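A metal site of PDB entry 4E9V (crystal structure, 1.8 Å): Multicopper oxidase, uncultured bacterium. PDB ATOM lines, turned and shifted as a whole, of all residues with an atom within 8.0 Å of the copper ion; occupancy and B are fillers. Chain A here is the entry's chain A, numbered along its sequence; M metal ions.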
ATOM      1  N   ILE A  10      15.669 -32.804   4.997  1.00  0.00           N
ATOM      2  CA  ILE A  10      16.939 -32.468   4.395  1.00  0.00           C
ATOM      3  C   ILE A  10      18.001 -32.896   5.416  1.00  0.00           C
ATOM      4  O   ILE A  10      17.953 -32.468   6.571  1.00  0.00           O
ATOM      5  CB  ILE A  10      17.060 -30.999   4.008  1.00  0.00           C
ATOM      6  CG1 ILE A  10      15.796 -30.407   3.373  1.00  0.00           C
ATOM      7  CG2 ILE A  10      18.253 -30.753   3.087  1.00  0.00           C
ATOM      8  CD1 ILE A  10      15.885 -28.895   3.193  1.00  0.00           C
ATOM      9  N   PHE A  26      23.655 -32.746   0.592  1.00  0.00           N
ATOM     10  CA  PHE A  26      22.463 -32.350   1.311  1.00  0.00           C
ATOM     11  C   PHE A  26      21.293 -33.067   0.659  1.00  0.00           C
ATOM     12  O   PHE A  26      20.592 -32.530  -0.184  1.00  0.00           O
ATOM     13  CB  PHE A  26      22.259 -30.845   1.315  1.00  0.00           C
ATOM     14  CG  PHE A  26      23.313 -30.023   2.031  1.00  0.00           C
ATOM     15  CD1 PHE A  26      23.622 -30.266   3.359  1.00  0.00           C
ATOM     16  CD2 PHE A  26      23.976 -29.004   1.367  1.00  0.00           C
ATOM     17  CE1 PHE A  26      24.573 -29.525   4.029  1.00  0.00           C
ATOM     18  CE2 PHE A  26      24.930 -28.244   2.026  1.00  0.00           C
ATOM     19  CZ  PHE A  26      25.227 -28.494   3.358  1.00  0.00           C
ATOM     20  N   PHE A  28      17.793 -34.763   0.037  1.00  0.00           N
ATOM     21  CA  PHE A  28      16.390 -34.811   0.438  1.00  0.00           C
ATOM     22  C   PHE A  28      16.077 -36.229   0.896  1.00  0.00           C
ATOM     23  O   PHE A  28      16.359 -37.166   0.151  1.00  0.00           O
ATOM     24  CB  PHE A  28      15.518 -34.380  -0.734  1.00  0.00           C
ATOM     25  CG  PHE A  28      15.678 -32.905  -1.063  1.00  0.00           C
ATOM     26  CD1 PHE A  28      15.257 -31.958  -0.137  1.00  0.00           C
ATOM     27  CD2 PHE A  28      16.235 -32.471  -2.249  1.00  0.00           C
ATOM     28  CE1 PHE A  28      15.384 -30.604  -0.395  1.00  0.00           C
ATOM     29  CE2 PHE A  28      16.332 -31.123  -2.536  1.00  0.00           C
ATOM     30  CZ  PHE A  28      15.893 -30.191  -1.615  1.00  0.00           C
ATOM     31  N   ASN A  51      14.358 -29.137   7.839  1.00  0.00           N
ATOM     32  CA  ASN A  51      15.781 -29.000   7.594  1.00  0.00           C
ATOM     33  C   ASN A  51      16.629 -29.598   8.708  1.00  0.00           C
ATOM     34  O   ASN A  51      16.842 -28.938   9.729  1.00  0.00           O
ATOM     35  CB  ASN A  51      16.101 -27.508   7.442  1.00  0.00           C
ATOM     36  CG  ASN A  51      17.562 -27.292   7.075  1.00  0.00           C
ATOM     37  OD1 ASN A  51      18.351 -28.233   6.984  1.00  0.00           O
ATOM     38  ND2 ASN A  51      17.896 -26.025   6.865  1.00  0.00           N
ATOM     39  N   THR A  53      19.847 -30.164   8.537  1.00  0.00           N
ATOM     40  CA  THR A  53      21.260 -29.910   8.266  1.00  0.00           C
ATOM     41  C   THR A  53      21.691 -28.618   8.973  1.00  0.00           C
ATOM     42  O   THR A  53      20.858 -27.944   9.577  1.00  0.00           O
ATOM     43  CB  THR A  53      21.529 -29.752   6.753  1.00  0.00           C
ATOM     44  OG1 THR A  53      21.152 -28.417   6.347  1.00  0.00           O
ATOM     45  CG2 THR A  53      20.658 -30.716   5.953  1.00  0.00           C
ATOM     46  N   LEU A  55      22.735 -25.823   7.535  1.00  0.00           N
ATOM     47  CA  LEU A  55      22.683 -24.639   6.687  1.00  0.00           C
ATOM     48  C   LEU A  55      21.274 -24.401   6.200  1.00  0.00           C
ATOM     49  O   LEU A  55      20.476 -25.345   6.201  1.00  0.00           O
ATOM     50  CB  LEU A  55      23.597 -24.788   5.465  1.00  0.00           C
ATOM     51  CG  LEU A  55      25.101 -24.827   5.730  1.00  0.00           C
ATOM     52  CD1 LEU A  55      25.837 -25.237   4.466  1.00  0.00           C
ATOM     53  CD2 LEU A  55      25.575 -23.484   6.261  1.00  0.00           C
ATOM     54  N   PRO A  56      20.961 -23.188   5.774  1.00  0.00           N
ATOM     55  CA  PRO A  56      19.647 -22.865   5.255  1.00  0.00           C
ATOM     56  C   PRO A  56      19.466 -23.413   3.827  1.00  0.00           C
ATOM     57  O   PRO A  56      20.416 -23.541   3.052  1.00  0.00           O
ATOM     58  CB  PRO A  56      19.603 -21.343   5.194  1.00  0.00           C
ATOM     59  CG  PRO A  56      20.897 -20.858   5.740  1.00  0.00           C
ATOM     60  CD  PRO A  56      21.854 -22.002   5.757  1.00  0.00           C
ATOM     61  N   HIS A  57      18.213 -23.754   3.546  1.00  0.00           N
ATOM     62  CA  HIS A  57      17.766 -24.255   2.259  1.00  0.00           C
ATOM     63  C   HIS A  57      16.359 -23.722   1.996  1.00  0.00           C
ATOM     64  O   HIS A  57      15.708 -23.117   2.842  1.00  0.00           O
ATOM     65  CB  HIS A  57      17.773 -25.789   2.209  1.00  0.00           C
ATOM     66  CG  HIS A  57      19.047 -26.445   2.641  1.00  0.00           C
ATOM     67  ND1 HIS A  57      20.157 -26.572   1.854  1.00  0.00           N
ATOM     68  CD2 HIS A  57      19.410 -27.003   3.817  1.00  0.00           C
ATOM     69  CE1 HIS A  57      21.131 -27.183   2.476  1.00  0.00           C
ATOM     70  NE2 HIS A  57      20.695 -27.457   3.704  1.00  0.00           N
ATOM     71  N   THR A  58      15.844 -23.966   0.805  1.00  0.00           N
ATOM     72  CA  THR A  58      14.461 -23.900   0.391  1.00  0.00           C
ATOM     73  C   THR A  58      14.220 -25.065  -0.588  1.00  0.00           C
ATOM     74  O   THR A  58      15.177 -25.742  -0.955  1.00  0.00           O
ATOM     75  CB  THR A  58      14.086 -22.610  -0.350  1.00  0.00           C
ATOM     76  OG1 THR A  58      14.892 -22.574  -1.541  1.00  0.00           O
ATOM     77  CG2 THR A  58      14.393 -21.361   0.470  1.00  0.00           C
ATOM     78  N   ILE A  59      12.985 -25.253  -1.012  1.00  0.00           N
ATOM     79  CA  ILE A  59      12.730 -26.088  -2.194  1.00  0.00           C
ATOM     80  C   ILE A  59      11.929 -25.252  -3.192  1.00  0.00           C
ATOM     81  O   ILE A  59      10.879 -24.705  -2.886  1.00  0.00           O
ATOM     82  CB  ILE A  59      11.997 -27.394  -1.877  1.00  0.00           C
ATOM     83  CG1 ILE A  59      12.698 -28.219  -0.784  1.00  0.00           C
ATOM     84  CG2 ILE A  59      11.781 -28.230  -3.145  1.00  0.00           C
ATOM     85  CD1 ILE A  59      11.936 -29.517  -0.499  1.00  0.00           C
ATOM     86  N   ILE A  83      14.767 -21.554   4.786  1.00  0.00           N
ATOM     87  CA  ILE A  83      14.467 -22.486   5.868  1.00  0.00           C
ATOM     88  C   ILE A  83      15.733 -22.716   6.670  1.00  0.00           C
ATOM     89  O   ILE A  83      16.666 -23.373   6.206  1.00  0.00           O
ATOM     90  CB  ILE A  83      13.912 -23.809   5.318  1.00  0.00           C
ATOM     91  CG1 ILE A  83      12.758 -23.593   4.347  1.00  0.00           C
ATOM     92  CG2 ILE A  83      13.550 -24.738   6.465  1.00  0.00           C
ATOM     93  CD1 ILE A  83      12.250 -24.821   3.626  1.00  0.00           C
ATOM     94  N   HIS A 104      14.352 -28.536  -6.515  1.00  0.00           N
ATOM     95  CA  HIS A 104      15.721 -28.375  -6.068  1.00  0.00           C
ATOM     96  C   HIS A 104      15.848 -27.219  -5.078  1.00  0.00           C
ATOM     97  O   HIS A 104      15.004 -26.339  -4.974  1.00  0.00           O
ATOM     98  CB  HIS A 104      16.694 -28.133  -7.232  1.00  0.00           C
ATOM     99  CG  HIS A 104      16.380 -26.963  -8.105  1.00  0.00           C
ATOM    100  ND1 HIS A 104      16.739 -25.672  -7.794  1.00  0.00           N
ATOM    101  CD2 HIS A 104      15.739 -26.878  -9.303  1.00  0.00           C
ATOM    102  CE1 HIS A 104      16.327 -24.847  -8.747  1.00  0.00           C
ATOM    103  NE2 HIS A 104      15.721 -25.562  -9.670  1.00  0.00           N
ATOM    104  N   CYS A 105      16.952 -27.240  -4.326  1.00  0.00           N
ATOM    105  CA  CYS A 105      17.093 -26.112  -3.385  1.00  0.00           C
ATOM    106  C   CYS A 105      17.281 -24.843  -4.196  1.00  0.00           C
ATOM    107  O   CYS A 105      17.726 -24.928  -5.345  1.00  0.00           O
ATOM    108  CB  CYS A 105      18.272 -26.391  -2.459  1.00  0.00           C
ATOM    109  SG  CYS A 105      18.673 -25.092  -1.277  1.00  0.00           S
ATOM    110  N   HIS A 106      16.965 -23.688  -3.635  1.00  0.00           N
ATOM    111  CA  HIS A 106      17.168 -22.427  -4.331  1.00  0.00           C
ATOM    112  C   HIS A 106      17.967 -21.435  -3.476  1.00  0.00           C
ATOM    113  O   HIS A 106      17.919 -20.236  -3.730  1.00  0.00           O
ATOM    114  CB  HIS A 106      15.843 -21.774  -4.747  1.00  0.00           C
ATOM    115  CG  HIS A 106      15.894 -21.188  -6.134  1.00  0.00           C
ATOM    116  ND1 HIS A 106      16.611 -20.040  -6.411  1.00  0.00           N
ATOM    117  CD2 HIS A 106      15.339 -21.586  -7.305  1.00  0.00           C
ATOM    118  CE1 HIS A 106      16.499 -19.754  -7.696  1.00  0.00           C
ATOM    119  NE2 HIS A 106      15.726 -20.669  -8.261  1.00  0.00           N
ATOM    120  N   VAL A 107      18.695 -21.962  -2.502  1.00  0.00           N
ATOM    121  CA  VAL A 107      19.672 -21.252  -1.715  1.00  0.00           C
ATOM    122  C   VAL A 107      21.087 -21.654  -2.173  1.00  0.00           C
ATOM    123  O   VAL A 107      21.279 -22.871  -2.279  1.00  0.00           O
ATOM    124  CB  VAL A 107      19.560 -21.598  -0.217  1.00  0.00           C
ATOM    125  CG1 VAL A 107      20.601 -20.827   0.586  1.00  0.00           C
ATOM    126  CG2 VAL A 107      18.157 -21.337   0.315  1.00  0.00           C
ATOM    127  N   ASN A 108      21.981 -20.704  -2.411  1.00  0.00           N
ATOM    128  CA  ASN A 108      23.379 -21.051  -2.698  1.00  0.00           C
ATOM    129  C   ASN A 108      23.478 -22.112  -3.790  1.00  0.00           C
ATOM    130  O   ASN A 108      24.267 -23.062  -3.709  1.00  0.00           O
ATOM    131  CB  ASN A 108      24.072 -21.557  -1.433  1.00  0.00           C
ATOM    132  CG  ASN A 108      24.516 -20.495  -0.443  1.00  0.00           C
ATOM    133  OD1 ASN A 108      24.712 -19.319  -0.768  1.00  0.00           O
ATOM    134  ND2 ASN A 108      24.699 -20.867   0.825  1.00  0.00           N
ATOM    135  N   VAL A 109      22.646 -21.955  -4.800  1.00  0.00           N
ATOM    136  CA  VAL A 109      22.391 -23.010  -5.773  1.00  0.00           C
ATOM    137  C   VAL A 109      23.630 -23.475  -6.533  1.00  0.00           C
ATOM    138  O   VAL A 109      23.696 -24.651  -6.903  1.00  0.00           O
ATOM    139  CB  VAL A 109      21.287 -22.569  -6.776  1.00  0.00           C
ATOM    140  CG1 VAL A 109      20.136 -21.941  -5.999  1.00  0.00           C
ATOM    141  CG2 VAL A 109      21.778 -21.590  -7.827  1.00  0.00           C
ATOM    142  N   GLU A 111      26.331 -24.115  -5.437  1.00  0.00           N
ATOM    143  CA  GLU A 111      26.918 -25.207  -4.669  1.00  0.00           C
ATOM    144  C   GLU A 111      25.871 -26.282  -4.360  1.00  0.00           C
ATOM    145  O   GLU A 111      26.109 -27.474  -4.571  1.00  0.00           O
ATOM    146  CB  GLU A 111      27.526 -24.708  -3.346  1.00  0.00           C
ATOM    147  CG  GLU A 111      28.279 -25.801  -2.603  1.00  0.00           C
ATOM    148  CD  GLU A 111      28.438 -25.566  -1.114  1.00  0.00           C
ATOM    149  OE1 GLU A 111      28.263 -24.406  -0.671  1.00  0.00           O
ATOM    150  OE2 GLU A 111      28.741 -26.535  -0.377  1.00  0.00           O
ATOM    151  N   HIS A 112      24.719 -25.851  -3.855  1.00  0.00           N
ATOM    152  CA  HIS A 112      23.748 -26.842  -3.370  1.00  0.00           C
ATOM    153  C   HIS A 112      23.173 -27.667  -4.507  1.00  0.00           C
ATOM    154  O   HIS A 112      22.994 -28.885  -4.380  1.00  0.00           O
ATOM    155  CB  HIS A 112      22.604 -26.177  -2.591  1.00  0.00           C
ATOM    156  CG  HIS A 112      23.038 -25.649  -1.254  1.00  0.00           C
ATOM    157  ND1 HIS A 112      22.148 -25.360  -0.233  1.00  0.00           N
ATOM    158  CD2 HIS A 112      24.280 -25.373  -0.792  1.00  0.00           C
ATOM    159  CE1 HIS A 112      22.839 -24.926   0.801  1.00  0.00           C
ATOM    160  NE2 HIS A 112      24.124 -24.924   0.499  1.00  0.00           N
ATOM    161  N   VAL A 113      22.864 -27.016  -5.625  1.00  0.00           N
ATOM    162  CA  VAL A 113      22.347 -27.790  -6.754  1.00  0.00           C
ATOM    163  C   VAL A 113      23.527 -28.318  -7.567  1.00  0.00           C
ATOM    164  O   VAL A 113      23.522 -29.427  -8.085  1.00  0.00           O
ATOM    165  CB  VAL A 113      21.389 -26.983  -7.644  1.00  0.00           C
ATOM    166  CG1 VAL A 113      20.901 -27.828  -8.822  1.00  0.00           C
ATOM    167  CG2 VAL A 113      20.208 -26.496  -6.821  1.00  0.00           C
ATOM    168  N   ARG A 116      25.846 -30.544  -4.377  1.00  0.00           N
ATOM    169  CA  ARG A 116      25.382 -31.139  -3.122  1.00  0.00           C
ATOM    170  C   ARG A 116      24.099 -31.954  -3.290  1.00  0.00           C
ATOM    171  O   ARG A 116      23.464 -32.315  -2.288  1.00  0.00           O
ATOM    172  CB  ARG A 116      25.166 -30.077  -2.039  1.00  0.00           C
ATOM    173  CG  ARG A 116      26.413 -29.289  -1.689  1.00  0.00           C
ATOM    174  CD  ARG A 116      27.524 -30.118  -1.082  1.00  0.00           C
ATOM    175  NE  ARG A 116      28.781 -29.385  -1.107  1.00  0.00           N
ATOM    176  CZ  ARG A 116      30.014 -29.850  -1.057  1.00  0.00           C
ATOM    177  NH1 ARG A 116      30.319 -31.138  -0.939  1.00  0.00           N
ATOM    178  NH2 ARG A 116      31.006 -28.966  -1.111  1.00  0.00           N
ATOM    179  N   MET A 118      21.059 -31.511  -4.209  1.00  0.00           N
ATOM    180  CA  MET A 118      19.756 -31.052  -3.719  1.00  0.00           C
ATOM    181  C   MET A 118      18.715 -30.955  -4.815  1.00  0.00           C
ATOM    182  O   MET A 118      18.285 -29.862  -5.202  1.00  0.00           O
ATOM    183  CB  MET A 118      19.926 -29.696  -3.008  1.00  0.00           C
ATOM    184  CG  MET A 118      20.977 -29.793  -1.884  1.00  0.00           C
ATOM    185  SD  MET A 118      20.611 -28.527  -0.634  1.00  0.00           S
ATOM    186  CE  MET A 118      19.066 -29.165   0.025  1.00  0.00           C
HETATM  187 CU    CU M   1      20.338 -25.846  -0.110  1.00  0.00          CU
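The backbone carbonyl oxygen of His 57 lies within hydrogen-bond range of the backbone NH of Ile 83 (2.7 Å). SG of Cys 105 sits close to O of Thr 58 (3.6 Å). The backbone carbonyl oxygen of Leu 55 sits close to a ring nitrogen (NE2) of His 57, 3.3 Å away. NE2 of His 57 lies within hydrogen-bond range of OG1 of Thr 53 (2.8 Å). The backbone carbonyl oxygen (O) of Val 107 lies close to a ring nitrogen (ND1) of His 112 (3.3 Å). N of Val 107 sits close to SG of Cys 105 (3.4 Å).
Residues that only touch the copper ion: Pro 56 and Val 107. Of the 22 residues printed, 6 come within 4 Å of the copper ion.
The copper ion is bound by ND1 of His 112 (1.9 Å), ND1 of His 57 (2.1 Å), SG of Cys 105 (2.2 Å) and SD of Met 118 (2.7 Å). The copper ion has four donor atoms within binding distance.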
